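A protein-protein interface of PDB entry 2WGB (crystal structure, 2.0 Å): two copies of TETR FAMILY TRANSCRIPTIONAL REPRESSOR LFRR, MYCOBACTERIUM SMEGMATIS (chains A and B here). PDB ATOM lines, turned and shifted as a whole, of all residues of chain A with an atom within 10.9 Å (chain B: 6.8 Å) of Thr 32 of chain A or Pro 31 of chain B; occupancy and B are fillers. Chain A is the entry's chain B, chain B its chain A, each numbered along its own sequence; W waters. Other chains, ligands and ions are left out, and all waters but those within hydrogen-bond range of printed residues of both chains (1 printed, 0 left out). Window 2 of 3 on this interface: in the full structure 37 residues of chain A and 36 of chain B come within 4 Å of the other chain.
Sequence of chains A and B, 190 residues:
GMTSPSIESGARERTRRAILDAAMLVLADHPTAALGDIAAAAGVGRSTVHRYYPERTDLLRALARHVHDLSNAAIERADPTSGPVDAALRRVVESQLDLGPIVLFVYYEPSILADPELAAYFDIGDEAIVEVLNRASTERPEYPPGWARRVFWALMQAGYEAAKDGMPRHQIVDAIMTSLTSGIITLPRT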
ATOM      1  N   ALA A  23     -23.184 -13.963  36.731  1.00  0.00           N
ATOM      2  CA  ALA A  23     -22.409 -12.957  36.022  1.00  0.00           C
ATOM      3  C   ALA A  23     -21.176 -12.530  36.814  1.00  0.00           C
ATOM      4  O   ALA A  23     -20.063 -12.519  36.282  1.00  0.00           O
ATOM      5  CB  ALA A  23     -23.285 -11.746  35.695  1.00  0.00           C
ATOM      6  N   MET A  24     -21.379 -12.179  38.083  1.00  0.00           N
ATOM      7  CA  MET A  24     -20.282 -11.763  38.955  1.00  0.00           C
ATOM      8  C   MET A  24     -19.191 -12.822  38.992  1.00  0.00           C
ATOM      9  O   MET A  24     -18.004 -12.516  38.869  1.00  0.00           O
ATOM     10  CB  MET A  24     -20.786 -11.494  40.379  1.00  0.00           C
ATOM     11  CG  MET A  24     -21.539 -10.194  40.548  1.00  0.00           C
ATOM     12  SD  MET A  24     -22.147  -9.918  42.225  1.00  0.00           S
ATOM     13  CE  MET A  24     -20.638 -10.150  43.157  1.00  0.00           C
ATOM     14  N   LEU A  25     -19.605 -14.071  39.164  1.00  0.00           N
ATOM     15  CA  LEU A  25     -18.673 -15.185  39.258  1.00  0.00           C
ATOM     16  C   LEU A  25     -17.936 -15.407  37.941  1.00  0.00           C
ATOM     17  O   LEU A  25     -16.710 -15.524  37.911  1.00  0.00           O
ATOM     18  CB  LEU A  25     -19.416 -16.459  39.661  1.00  0.00           C
ATOM     19  CG  LEU A  25     -18.555 -17.711  39.800  1.00  0.00           C
ATOM     20  CD1 LEU A  25     -17.384 -17.446  40.733  1.00  0.00           C
ATOM     21  CD2 LEU A  25     -19.385 -18.889  40.288  1.00  0.00           C
ATOM     22  N   VAL A  26     -18.698 -15.458  36.856  1.00  0.00           N
ATOM     23  CA  VAL A  26     -18.148 -15.764  35.543  1.00  0.00           C
ATOM     24  C   VAL A  26     -17.285 -14.633  34.988  1.00  0.00           C
ATOM     25  O   VAL A  26     -16.138 -14.849  34.599  1.00  0.00           O
ATOM     26  CB  VAL A  26     -19.275 -16.087  34.545  1.00  0.00           C
ATOM     27  CG1 VAL A  26     -18.714 -16.257  33.140  1.00  0.00           C
ATOM     28  CG2 VAL A  26     -20.018 -17.339  34.986  1.00  0.00           C
ATOM     29  N   LEU A  27     -17.838 -13.427  34.952  1.00  0.00           N
ATOM     30  CA  LEU A  27     -17.145 -12.299  34.338  1.00  0.00           C
ATOM     31  C   LEU A  27     -15.865 -11.922  35.079  1.00  0.00           C
ATOM     32  O   LEU A  27     -14.947 -11.349  34.489  1.00  0.00           O
ATOM     33  CB  LEU A  27     -18.067 -11.086  34.229  1.00  0.00           C
ATOM     34  CG  LEU A  27     -19.225 -11.251  33.244  1.00  0.00           C
ATOM     35  CD1 LEU A  27     -20.153 -10.045  33.294  1.00  0.00           C
ATOM     36  CD2 LEU A  27     -18.687 -11.478  31.834  1.00  0.00           C
ATOM     37  N   ALA A  28     -15.804 -12.253  36.365  1.00  0.00           N
ATOM     38  CA  ALA A  28     -14.632 -11.937  37.178  1.00  0.00           C
ATOM     39  C   ALA A  28     -13.341 -12.510  36.586  1.00  0.00           C
ATOM     40  O   ALA A  28     -12.294 -11.866  36.635  1.00  0.00           O
ATOM     41  CB  ALA A  28     -14.828 -12.421  38.612  1.00  0.00           C
ATOM     42  N   ASP A  29     -13.424 -13.711  36.018  1.00  0.00           N
ATOM     43  CA  ASP A  29     -12.252 -14.379  35.445  1.00  0.00           C
ATOM     44  C   ASP A  29     -12.263 -14.442  33.918  1.00  0.00           C
ATOM     45  O   ASP A  29     -11.218 -14.598  33.289  1.00  0.00           O
ATOM     46  CB  ASP A  29     -12.113 -15.796  36.003  1.00  0.00           C
ATOM     47  CG  ASP A  29     -11.732 -15.806  37.466  1.00  0.00           C
ATOM     48  OD1 ASP A  29     -11.237 -14.767  37.960  1.00  0.00           O
ATOM     49  OD2 ASP A  29     -11.929 -16.852  38.117  1.00  0.00           O
ATOM     50  N   HIS A  30     -13.449 -14.353  33.330  1.00  0.00           N
ATOM     51  CA  HIS A  30     -13.592 -14.367  31.879  1.00  0.00           C
ATOM     52  C   HIS A  30     -14.419 -13.158  31.475  1.00  0.00           C
ATOM     53  O   HIS A  30     -15.622 -13.277  31.267  1.00  0.00           O
ATOM     54  CB  HIS A  30     -14.282 -15.649  31.405  1.00  0.00           C
ATOM     55  CG  HIS A  30     -13.562 -16.909  31.784  1.00  0.00           C
ATOM     56  ND1 HIS A  30     -14.178 -18.142  31.792  1.00  0.00           N
ATOM     57  CD2 HIS A  30     -12.282 -17.128  32.169  1.00  0.00           C
ATOM     58  CE1 HIS A  30     -13.308 -19.067  32.160  1.00  0.00           C
ATOM     59  NE2 HIS A  30     -12.151 -18.477  32.398  1.00  0.00           N
ATOM     60  N   PRO A  31     -13.774 -11.982  31.379  1.00  0.00           N
ATOM     61  CA  PRO A  31     -14.442 -10.689  31.163  1.00  0.00           C
ATOM     62  C   PRO A  31     -15.195 -10.606  29.843  1.00  0.00           C
ATOM     63  O   PRO A  31     -16.154  -9.843  29.729  1.00  0.00           O
ATOM     64  CB  PRO A  31     -13.272  -9.689  31.163  1.00  0.00           C
ATOM     65  CG  PRO A  31     -12.066 -10.540  30.805  1.00  0.00           C
ATOM     66  CD  PRO A  31     -12.324 -11.810  31.559  1.00  0.00           C
ATOM     67  N   THR A  32     -14.778 -11.389  28.858  1.00  0.00           N
ATOM     68  CA  THR A  32     -15.414 -11.331  27.546  1.00  0.00           C
ATOM     69  C   THR A  32     -16.384 -12.488  27.341  1.00  0.00           C
ATOM     70  O   THR A  32     -16.781 -12.777  26.211  1.00  0.00           O
ATOM     71  CB  THR A  32     -14.370 -11.334  26.415  1.00  0.00           C
ATOM     72  OG1 THR A  32     -13.602 -12.541  26.483  1.00  0.00           O
ATOM     73  CG2 THR A  32     -13.436 -10.131  26.550  1.00  0.00           C
ATOM     74  N   ALA A  33     -16.772 -13.138  28.438  1.00  0.00           N
ATOM     75  CA  ALA A  33     -17.666 -14.298  28.371  1.00  0.00           C
ATOM     76  C   ALA A  33     -19.006 -13.954  27.731  1.00  0.00           C
ATOM     77  O   ALA A  33     -19.480 -12.825  27.832  1.00  0.00           O
ATOM     78  CB  ALA A  33     -17.878 -14.892  29.753  1.00  0.00           C
ATOM     79  N   ALA A  34     -19.620 -14.942  27.086  1.00  0.00           N
ATOM     80  CA  ALA A  34     -20.888 -14.740  26.393  1.00  0.00           C
ATOM     81  C   ALA A  34     -22.095 -15.008  27.288  1.00  0.00           C
ATOM     82  O   ALA A  34     -22.005 -15.749  28.268  1.00  0.00           O
ATOM     83  CB  ALA A  34     -20.953 -15.615  25.147  1.00  0.00           C
ATOM     84  N   LEU A  35     -23.227 -14.406  26.922  1.00  0.00           N
ATOM     85  CA  LEU A  35     -24.476 -14.537  27.670  1.00  0.00           C
ATOM     86  C   LEU A  35     -24.841 -15.987  27.980  1.00  0.00           C
ATOM     87  O   LEU A  35     -25.412 -16.280  29.031  1.00  0.00           O
ATOM     88  CB  LEU A  35     -25.621 -13.862  26.909  1.00  0.00           C
ATOM     89  CG  LEU A  35     -25.625 -12.332  26.858  1.00  0.00           C
ATOM     90  CD1 LEU A  35     -26.545 -11.829  25.755  1.00  0.00           C
ATOM     91  CD2 LEU A  35     -26.031 -11.749  28.204  1.00  0.00           C
ATOM     92  N   GLY A  36     -24.519 -16.890  27.060  1.00  0.00           N
ATOM     93  CA  GLY A  36     -24.798 -18.302  27.253  1.00  0.00           C
ATOM     94  C   GLY A  36     -23.995 -18.932  28.381  1.00  0.00           C
ATOM     95  O   GLY A  36     -24.473 -19.841  29.059  1.00  0.00           O
ATOM     96  N   ASP A  37     -22.768 -18.460  28.582  1.00  0.00           N
ATOM     97  CA  ASP A  37     -21.935 -18.967  29.669  1.00  0.00           C
ATOM     98  C   ASP A  37     -22.510 -18.534  31.007  1.00  0.00           C
ATOM     99  O   ASP A  37     -22.473 -19.278  31.985  1.00  0.00           O
ATOM    100  CB  ASP A  37     -20.499 -18.458  29.545  1.00  0.00           C
ATOM    101  CG  ASP A  37     -19.665 -19.287  28.595  1.00  0.00           C
ATOM    102  OD1 ASP A  37     -19.915 -20.509  28.490  1.00  0.00           O
ATOM    103  OD2 ASP A  37     -18.751 -18.717  27.962  1.00  0.00           O
ATOM    104  N   ILE A  38     -23.034 -17.316  31.048  1.00  0.00           N
ATOM    105  CA  ILE A  38     -23.621 -16.800  32.269  1.00  0.00           C
ATOM    106  C   ILE A  38     -24.900 -17.577  32.598  1.00  0.00           C
ATOM    107  O   ILE A  38     -25.148 -17.926  33.755  1.00  0.00           O
ATOM    108  CB  ILE A  38     -23.885 -15.285  32.158  1.00  0.00           C
ATOM    109  CG1 ILE A  38     -22.568 -14.548  31.881  1.00  0.00           C
ATOM    110  CG2 ILE A  38     -24.540 -14.763  33.420  1.00  0.00           C
ATOM    111  CD1 ILE A  38     -22.725 -13.068  31.652  1.00  0.00           C
ATOM    112  N   ARG A  56     -26.042  -7.985  25.457  1.00  0.00           N
ATOM    113  CA  ARG A  56     -25.033  -8.180  26.485  1.00  0.00           C
ATOM    114  C   ARG A  56     -24.810  -6.897  27.282  1.00  0.00           C
ATOM    115  O   ARG A  56     -24.577  -6.937  28.491  1.00  0.00           O
ATOM    116  CB  ARG A  56     -23.721  -8.654  25.858  1.00  0.00           C
ATOM    117  CG  ARG A  56     -22.667  -9.093  26.864  1.00  0.00           C
ATOM    118  CD  ARG A  56     -21.449  -9.681  26.165  1.00  0.00           C
ATOM    119  NE  ARG A  56     -20.489 -10.239  27.114  1.00  0.00           N
ATOM    120  CZ  ARG A  56     -19.429  -9.585  27.575  1.00  0.00           C
ATOM    121  NH1 ARG A  56     -19.187  -8.344  27.171  1.00  0.00           N
ATOM    122  NH2 ARG A  56     -18.609 -10.172  28.440  1.00  0.00           N
ATOM    123  N   THR A  57     -24.893  -5.758  26.602  1.00  0.00           N
ATOM    124  CA  THR A  57     -24.668  -4.476  27.260  1.00  0.00           C
ATOM    125  C   THR A  57     -25.731  -4.205  28.324  1.00  0.00           C
ATOM    126  O   THR A  57     -25.478  -3.497  29.299  1.00  0.00           O
ATOM    127  CB  THR A  57     -24.622  -3.314  26.247  1.00  0.00           C
ATOM    128  OG1 THR A  57     -25.864  -3.243  25.534  1.00  0.00           O
ATOM    129  CG2 THR A  57     -23.482  -3.516  25.261  1.00  0.00           C
ATOM    130  N   LEU A  59     -27.093  -6.508  30.330  1.00  0.00           N
ATOM    131  CA  LEU A  59     -26.692  -7.258  31.514  1.00  0.00           C
ATOM    132  C   LEU A  59     -25.554  -6.563  32.244  1.00  0.00           C
ATOM    133  O   LEU A  59     -25.583  -6.431  33.465  1.00  0.00           O
ATOM    134  CB  LEU A  59     -26.294  -8.690  31.141  1.00  0.00           C
ATOM    135  CG  LEU A  59     -25.843  -9.591  32.298  1.00  0.00           C
ATOM    136  CD1 LEU A  59     -26.813  -9.509  33.467  1.00  0.00           C
ATOM    137  CD2 LEU A  59     -25.689 -11.030  31.838  1.00  0.00           C
ATOM    138  N   LEU A  60     -24.546  -6.128  31.493  1.00  0.00           N
ATOM    139  CA  LEU A  60     -23.428  -5.379  32.065  1.00  0.00           C
ATOM    140  C   LEU A  60     -23.919  -4.159  32.843  1.00  0.00           C
ATOM    141  O   LEU A  60     -23.407  -3.852  33.920  1.00  0.00           O
ATOM    142  CB  LEU A  60     -22.452  -4.944  30.968  1.00  0.00           C
ATOM    143  CG  LEU A  60     -21.263  -5.867  30.687  1.00  0.00           C
ATOM    144  CD1 LEU A  60     -21.635  -7.315  30.944  1.00  0.00           C
ATOM    145  CD2 LEU A  60     -20.776  -5.679  29.258  1.00  0.00           C
ATOM    146  N   LEU A  63     -25.423  -5.326  36.187  1.00  0.00           N
ATOM    147  CA  LEU A  63     -24.339  -5.827  37.024  1.00  0.00           C
ATOM    148  C   LEU A  63     -23.536  -4.685  37.647  1.00  0.00           C
ATOM    149  O   LEU A  63     -23.209  -4.713  38.831  1.00  0.00           O
ATOM    150  CB  LEU A  63     -23.407  -6.729  36.212  1.00  0.00           C
ATOM    151  CG  LEU A  63     -22.280  -7.398  37.003  1.00  0.00           C
ATOM    152  CD1 LEU A  63     -22.852  -8.358  38.037  1.00  0.00           C
ATOM    153  CD2 LEU A  63     -21.321  -8.121  36.066  1.00  0.00           C
ATOM    154  N   ILE A 102     -14.425  -8.421  40.348  1.00  0.00           N
ATOM    155  CA  ILE A 102     -15.593  -7.892  39.652  1.00  0.00           C
ATOM    156  C   ILE A 102     -15.723  -6.387  39.915  1.00  0.00           C
ATOM    157  O   ILE A 102     -16.236  -5.634  39.081  1.00  0.00           O
ATOM    158  CB  ILE A 102     -16.891  -8.644  40.051  1.00  0.00           C
ATOM    159  CG1 ILE A 102     -17.959  -8.487  38.965  1.00  0.00           C
ATOM    160  CG2 ILE A 102     -17.399  -8.188  41.424  1.00  0.00           C
ATOM    161  CD1 ILE A 102     -17.615  -9.210  37.669  1.00  0.00           C
ATOM    162  N   PHE A 105     -13.716  -4.856  37.232  1.00  0.00           N
ATOM    163  CA  PHE A 105     -14.386  -5.131  35.971  1.00  0.00           C
ATOM    164  C   PHE A 105     -15.422  -4.059  35.617  1.00  0.00           C
ATOM    165  O   PHE A 105     -15.406  -3.522  34.508  1.00  0.00           O
ATOM    166  CB  PHE A 105     -15.043  -6.515  35.982  1.00  0.00           C
ATOM    167  CG  PHE A 105     -15.859  -6.805  34.748  1.00  0.00           C
ATOM    168  CD1 PHE A 105     -17.241  -6.676  34.764  1.00  0.00           C
ATOM    169  CD2 PHE A 105     -15.239  -7.195  33.567  1.00  0.00           C
ATOM    170  CE1 PHE A 105     -17.995  -6.936  33.625  1.00  0.00           C
ATOM    171  CE2 PHE A 105     -15.984  -7.459  32.425  1.00  0.00           C
ATOM    172  CZ  PHE A 105     -17.367  -7.328  32.454  1.00  0.00           C
ATOM    173  N   GLU A 109     -14.484  -1.216  32.384  1.00  0.00           N
ATOM    174  CA  GLU A 109     -15.145  -1.539  31.124  1.00  0.00           C
ATOM    175  C   GLU A 109     -15.529  -0.297  30.308  1.00  0.00           C
ATOM    176  O   GLU A 109     -16.298   0.549  30.773  1.00  0.00           O
ATOM    177  CB  GLU A 109     -16.392  -2.378  31.408  1.00  0.00           C
ATOM    178  CG  GLU A 109     -17.198  -2.757  30.177  1.00  0.00           C
ATOM    179  CD  GLU A 109     -16.572  -3.898  29.392  1.00  0.00           C
ATOM    180  OE1 GLU A 109     -15.524  -4.420  29.830  1.00  0.00           O
ATOM    181  OE2 GLU A 109     -17.127  -4.272  28.338  1.00  0.00           O
ATOM    182  N   PRO A 110     -15.004  -0.197  29.076  1.00  0.00           N
ATOM    183  CA  PRO A 110     -15.261   0.924  28.164  1.00  0.00           C
ATOM    184  C   PRO A 110     -16.754   1.210  28.016  1.00  0.00           C
ATOM    185  O   PRO A 110     -17.156   2.376  28.019  1.00  0.00           O
ATOM    186  CB  PRO A 110     -14.681   0.422  26.831  1.00  0.00           C
ATOM    187  CG  PRO A 110     -14.568  -1.081  27.006  1.00  0.00           C
ATOM    188  CD  PRO A 110     -14.163  -1.217  28.432  1.00  0.00           C
ATOM    189  N   SER A 111     -17.557   0.157  27.885  1.00  0.00           N
ATOM    190  CA  SER A 111     -19.011   0.287  27.824  1.00  0.00           C
ATOM    191  C   SER A 111     -19.536   1.250  28.883  1.00  0.00           C
ATOM    192  O   SER A 111     -20.167   2.258  28.561  1.00  0.00           O
ATOM    193  CB  SER A 111     -19.678  -1.082  27.993  1.00  0.00           C
ATOM    194  OG  SER A 111     -21.011  -0.954  28.464  1.00  0.00           O
ATOM    195  N   VAL B  26      -8.970  -1.984  19.289  1.00  0.00           N
ATOM    196  CA  VAL B  26     -10.292  -2.616  19.231  1.00  0.00           C
ATOM    197  C   VAL B  26     -10.346  -3.847  20.146  1.00  0.00           C
ATOM    198  O   VAL B  26     -11.298  -4.029  20.922  1.00  0.00           O
ATOM    199  CB  VAL B  26     -10.673  -2.998  17.775  1.00  0.00           C
ATOM    200  CG1 VAL B  26     -11.928  -3.872  17.749  1.00  0.00           C
ATOM    201  CG2 VAL B  26     -10.879  -1.734  16.930  1.00  0.00           C
ATOM    202  N   LEU B  27      -9.315  -4.683  20.074  1.00  0.00           N
ATOM    203  CA  LEU B  27      -9.281  -5.926  20.862  1.00  0.00           C
ATOM    204  C   LEU B  27      -9.218  -5.665  22.363  1.00  0.00           C
ATOM    205  O   LEU B  27      -9.664  -6.481  23.167  1.00  0.00           O
ATOM    206  CB  LEU B  27      -8.101  -6.807  20.440  1.00  0.00           C
ATOM    207  CG  LEU B  27      -8.343  -7.711  19.233  1.00  0.00           C
ATOM    208  CD1 LEU B  27      -8.910  -6.912  18.100  1.00  0.00           C
ATOM    209  CD2 LEU B  27      -7.050  -8.418  18.794  1.00  0.00           C
ATOM    210  N   ALA B  28      -8.636  -4.538  22.742  1.00  0.00           N
ATOM    211  CA  ALA B  28      -8.615  -4.147  24.138  1.00  0.00           C
ATOM    212  C   ALA B  28     -10.038  -3.970  24.681  1.00  0.00           C
ATOM    213  O   ALA B  28     -10.296  -4.240  25.855  1.00  0.00           O
ATOM    214  CB  ALA B  28      -7.825  -2.867  24.307  1.00  0.00           C
ATOM    215  N   ASP B  29     -10.953  -3.525  23.818  1.00  0.00           N
ATOM    216  CA  ASP B  29     -12.300  -3.130  24.240  1.00  0.00           C
ATOM    217  C   ASP B  29     -13.403  -4.048  23.737  1.00  0.00           C
ATOM    218  O   ASP B  29     -14.547  -3.947  24.176  1.00  0.00           O
ATOM    219  CB  ASP B  29     -12.603  -1.707  23.762  1.00  0.00           C
ATOM    220  CG  ASP B  29     -11.948  -0.659  24.620  1.00  0.00           C
ATOM    221  OD1 ASP B  29     -11.623  -0.968  25.784  1.00  0.00           O
ATOM    222  OD2 ASP B  29     -11.766   0.475  24.135  1.00  0.00           O
ATOM    223  N   HIS B  30     -13.074  -4.926  22.801  1.00  0.00           N
ATOM    224  CA  HIS B  30     -14.068  -5.844  22.263  1.00  0.00           C
ATOM    225  C   HIS B  30     -13.513  -7.258  22.126  1.00  0.00           C
ATOM    226  O   HIS B  30     -12.410  -7.452  21.621  1.00  0.00           O
ATOM    227  CB  HIS B  30     -14.591  -5.329  20.921  1.00  0.00           C
ATOM    228  CG  HIS B  30     -15.066  -3.910  20.971  1.00  0.00           C
ATOM    229  ND1 HIS B  30     -16.339  -3.565  21.370  1.00  0.00           N
ATOM    230  CD2 HIS B  30     -14.432  -2.747  20.689  1.00  0.00           C
ATOM    231  CE1 HIS B  30     -16.471  -2.251  21.327  1.00  0.00           C
ATOM    232  NE2 HIS B  30     -15.329  -1.731  20.914  1.00  0.00           N
ATOM    233  N   PRO B  31     -14.285  -8.255  22.578  1.00  0.00           N
ATOM    234  CA  PRO B  31     -13.853  -9.655  22.492  1.00  0.00           C
ATOM    235  C   PRO B  31     -13.335  -9.975  21.093  1.00  0.00           C
ATOM    236  O   PRO B  31     -12.197 -10.424  20.926  1.00  0.00           O
ATOM    237  CB  PRO B  31     -15.142 -10.433  22.766  1.00  0.00           C
ATOM    238  CG  PRO B  31     -15.981  -9.502  23.582  1.00  0.00           C
ATOM    239  CD  PRO B  31     -15.664  -8.122  23.082  1.00  0.00           C
ATOM    240  N   THR B  32     -14.175  -9.728  20.094  1.00  0.00           N
ATOM    241  CA  THR B  32     -13.799  -9.947  18.705  1.00  0.00           C
ATOM    242  C   THR B  32     -13.474  -8.622  18.033  1.00  0.00           C
ATOM    243  O   THR B  32     -13.968  -7.571  18.437  1.00  0.00           O
ATOM    244  CB  THR B  32     -14.938 -10.604  17.918  1.00  0.00           C
ATOM    245  OG1 THR B  32     -15.860  -9.596  17.483  1.00  0.00           O
ATOM    246  CG2 THR B  32     -15.664 -11.622  18.785  1.00  0.00           C
ATOM    247  N   ALA B  33     -12.637  -8.679  17.005  1.00  0.00           N
ATOM    248  CA  ALA B  33     -12.321  -7.502  16.211  1.00  0.00           C
ATOM    249  C   ALA B  33     -13.197  -7.473  14.970  1.00  0.00           C
ATOM    250  O   ALA B  33     -12.813  -8.001  13.922  1.00  0.00           O
ATOM    251  CB  ALA B  33     -10.867  -7.525  15.811  1.00  0.00           C
ATOM    252  N   ILE B 112      -7.697  -6.431  33.867  1.00  0.00           N
ATOM    253  CA  ILE B 112      -9.005  -7.010  34.134  1.00  0.00           C
ATOM    254  C   ILE B 112      -9.859  -7.179  32.880  1.00  0.00           C
ATOM    255  O   ILE B 112     -10.667  -8.102  32.802  1.00  0.00           O
ATOM    256  CB  ILE B 112      -9.795  -6.163  35.178  1.00  0.00           C
ATOM    257  CG1 ILE B 112     -11.069  -6.895  35.616  1.00  0.00           C
ATOM    258  CG2 ILE B 112     -10.133  -4.779  34.616  1.00  0.00           C
ATOM    259  CD1 ILE B 112     -10.827  -8.005  36.617  1.00  0.00           C
ATOM    260  N   LEU B 113      -9.697  -6.293  31.901  1.00  0.00           N
ATOM    261  CA  LEU B 113     -10.514  -6.380  30.689  1.00  0.00           C
ATOM    262  C   LEU B 113      -9.924  -7.274  29.594  1.00  0.00           C
ATOM    263  O   LEU B 113     -10.639  -7.688  28.682  1.00  0.00           O
ATOM    264  CB  LEU B 113     -10.787  -4.986  30.119  1.00  0.00           C
ATOM    265  CG  LEU B 113     -11.596  -4.060  31.028  1.00  0.00           C
ATOM    266  CD1 LEU B 113     -11.726  -2.684  30.403  1.00  0.00           C
ATOM    267  CD2 LEU B 113     -12.968  -4.663  31.328  1.00  0.00           C
ATOM    268  N   ALA B 114      -8.631  -7.575  29.688  1.00  0.00           N
ATOM    269  CA  ALA B 114      -7.972  -8.401  28.669  1.00  0.00           C
ATOM    270  C   ALA B 114      -8.531  -9.827  28.661  1.00  0.00           C
ATOM    271  O   ALA B 114      -8.531 -10.510  29.689  1.00  0.00           O
ATOM    272  CB  ALA B 114      -6.473  -8.429  28.896  1.00  0.00           C
ATOM    273  N   ASP B 115      -9.014 -10.259  27.497  1.00  0.00           N
ATOM    274  CA  ASP B 115      -9.431 -11.644  27.274  1.00  0.00           C
ATOM    275  C   ASP B 115      -8.226 -12.528  27.568  1.00  0.00           C
ATOM    276  O   ASP B 115      -7.190 -12.391  26.926  1.00  0.00           O
ATOM    277  CB  ASP B 115      -9.858 -11.810  25.808  1.00  0.00           C
ATOM    278  CG  ASP B 115     -10.271 -13.239  25.457  1.00  0.00           C
ATOM    279  OD1 ASP B 115      -9.878 -14.194  26.160  1.00  0.00           O
ATOM    280  OD2 ASP B 115     -10.993 -13.404  24.451  1.00  0.00           O
ATOM    281  N   PRO B 116      -8.356 -13.428  28.549  1.00  0.00           N
ATOM    282  CA  PRO B 116      -7.211 -14.232  28.986  1.00  0.00           C
ATOM    283  C   PRO B 116      -6.605 -15.039  27.851  1.00  0.00           C
ATOM    284  O   PRO B 116      -5.397 -15.242  27.834  1.00  0.00           O
ATOM    285  CB  PRO B 116      -7.821 -15.177  30.029  1.00  0.00           C
ATOM    286  CG  PRO B 116      -9.066 -14.477  30.496  1.00  0.00           C
ATOM    287  CD  PRO B 116      -9.582 -13.740  29.305  1.00  0.00           C
ATOM    288  N   LEU B 118      -6.609 -14.225  24.617  1.00  0.00           N
ATOM    289  CA  LEU B 118      -5.836 -13.288  23.804  1.00  0.00           C
ATOM    290  C   LEU B 118      -4.473 -13.014  24.419  1.00  0.00           C
ATOM    291  O   LEU B 118      -3.462 -12.966  23.712  1.00  0.00           O
ATOM    292  CB  LEU B 118      -6.580 -11.964  23.633  1.00  0.00           C
ATOM    293  CG  LEU B 118      -7.495 -11.839  22.421  1.00  0.00           C
ATOM    294  CD1 LEU B 118      -8.140 -10.457  22.403  1.00  0.00           C
ATOM    295  CD2 LEU B 118      -6.698 -12.086  21.152  1.00  0.00           C
HETATM  296  O   HOH W   1     -10.294 -10.737  34.147  1.00  0.00           O
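The side-chain carboxylate (OD2) of Asp 115 of chain B is in hydrogen-bond range of the side-chain hydroxyl (OG1) of Thr 32 of chain A (3.4 Å).
O of Pro 31 of chain A is in hydrogen-bond range of NH2 of Arg 56 of chain A.
Pro 116 of chain B touches Asp 29 of chain A (CG to O, 3.5 Å). CG of Pro 31 of chain A touches O of Ile 112 of chain B, 3.4 Å away. Pro 31 of chain A touches Leu 113 of chain B (CG to O, 3.8 Å). CG of Pro 31 of chain A touches O of Ala 114 of chain B, 3.7 Å away. Thr 32 of chain A touches Pro 31 of chain B. Ile 112 of chain B touches Phe 105 of chain A. OE1 of Glu 109 of chain A touches CD2 of Leu 113 of chain B (3.0 Å). CG of Pro 110 of chain A touches OD1 of Asp 29 of chain B, at 3.2 Å. CD of Pro 110 of chain A touches CD1 of Leu 113 of chain B, 3.5 Å away.
Of chain B, only Pro 31 and Asp 115 come within 4 Å of Thr 32 of chain A. Of chain A, only Thr 32 comes within 4 Å of Pro 31 of chain B. Leu 27 of chain B touches none of the printed residues of chain A. Of chain A, only Thr 32 (3.4 Å) comes within 4 Å of Asp 115 of chain B. Of the printed residues of chain B, Asp 29 of chain A touches Pro 116 (3.5 Å). Of the printed residues of chain A, Asp 29 of chain B touches Pro 110 (3.2 Å). Of the printed residues of chain B, Glu 109 of chain A touches Leu 113 (3.0 Å). Printed residues of chain A within 4 Å of Ala 114 of chain B: Pro 31 (3.7 Å). Printed residues of chain A within 4 Å of Leu 113 of chain B: Pro 31 (3.8 Å), Glu 109 (3.0 Å) and Pro 110 (3.5 Å). Met 24 of chain A touches none of the printed residues of chain B. The nearest residue of chain B that does not touch Thr 32 of chain A is Leu 113 of chain B (4.3 Å). The nearest residue of chain A that does not touch Pro 31 of chain B is Arg 56 of chain A (4.9 Å).
Of the 14 printed residues of chain B, 7 touch a printed residue of chain A. Hydrophobic or aromatic side chains of chain B that line the printed part of chain A: Pro 31, Ile 112, Leu 113 and Pro 116. Of the 26 printed residues of chain A, 6 touch a printed residue of chain B. Printed residues of chain A that touch a printed residue of chain B: Asp 29, Pro 31, Thr 32, Phe 105, Glu 109 and Pro 110. Hydrophobic or aromatic side chains of chain A within 4 Å of the printed part of chain B: Pro 31 and Pro 110. Among the printed residues, no Asp or Glu carboxylate lies within 4 Å of a Lys or Arg side-chain nitrogen of the other chain.
Thr 32 of chain A touches Pro 31 of chain B, but with the chains exchanged Pro 31 of chain A does not touch Thr 32 of chain B (9.8 Å). Positions printed for both chains: 26, 27, 28, 29, 30, 31, 32 and 33. Of the 10 pairs that touch across the chains among the printed residues, none has its exchanged pair printed and touching as well.
Water W1 lies within hydrogen-bond range of O of Ile 112 of chain B (3.0 Å) and O of Ala 28 of chain A (3.4 Å).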
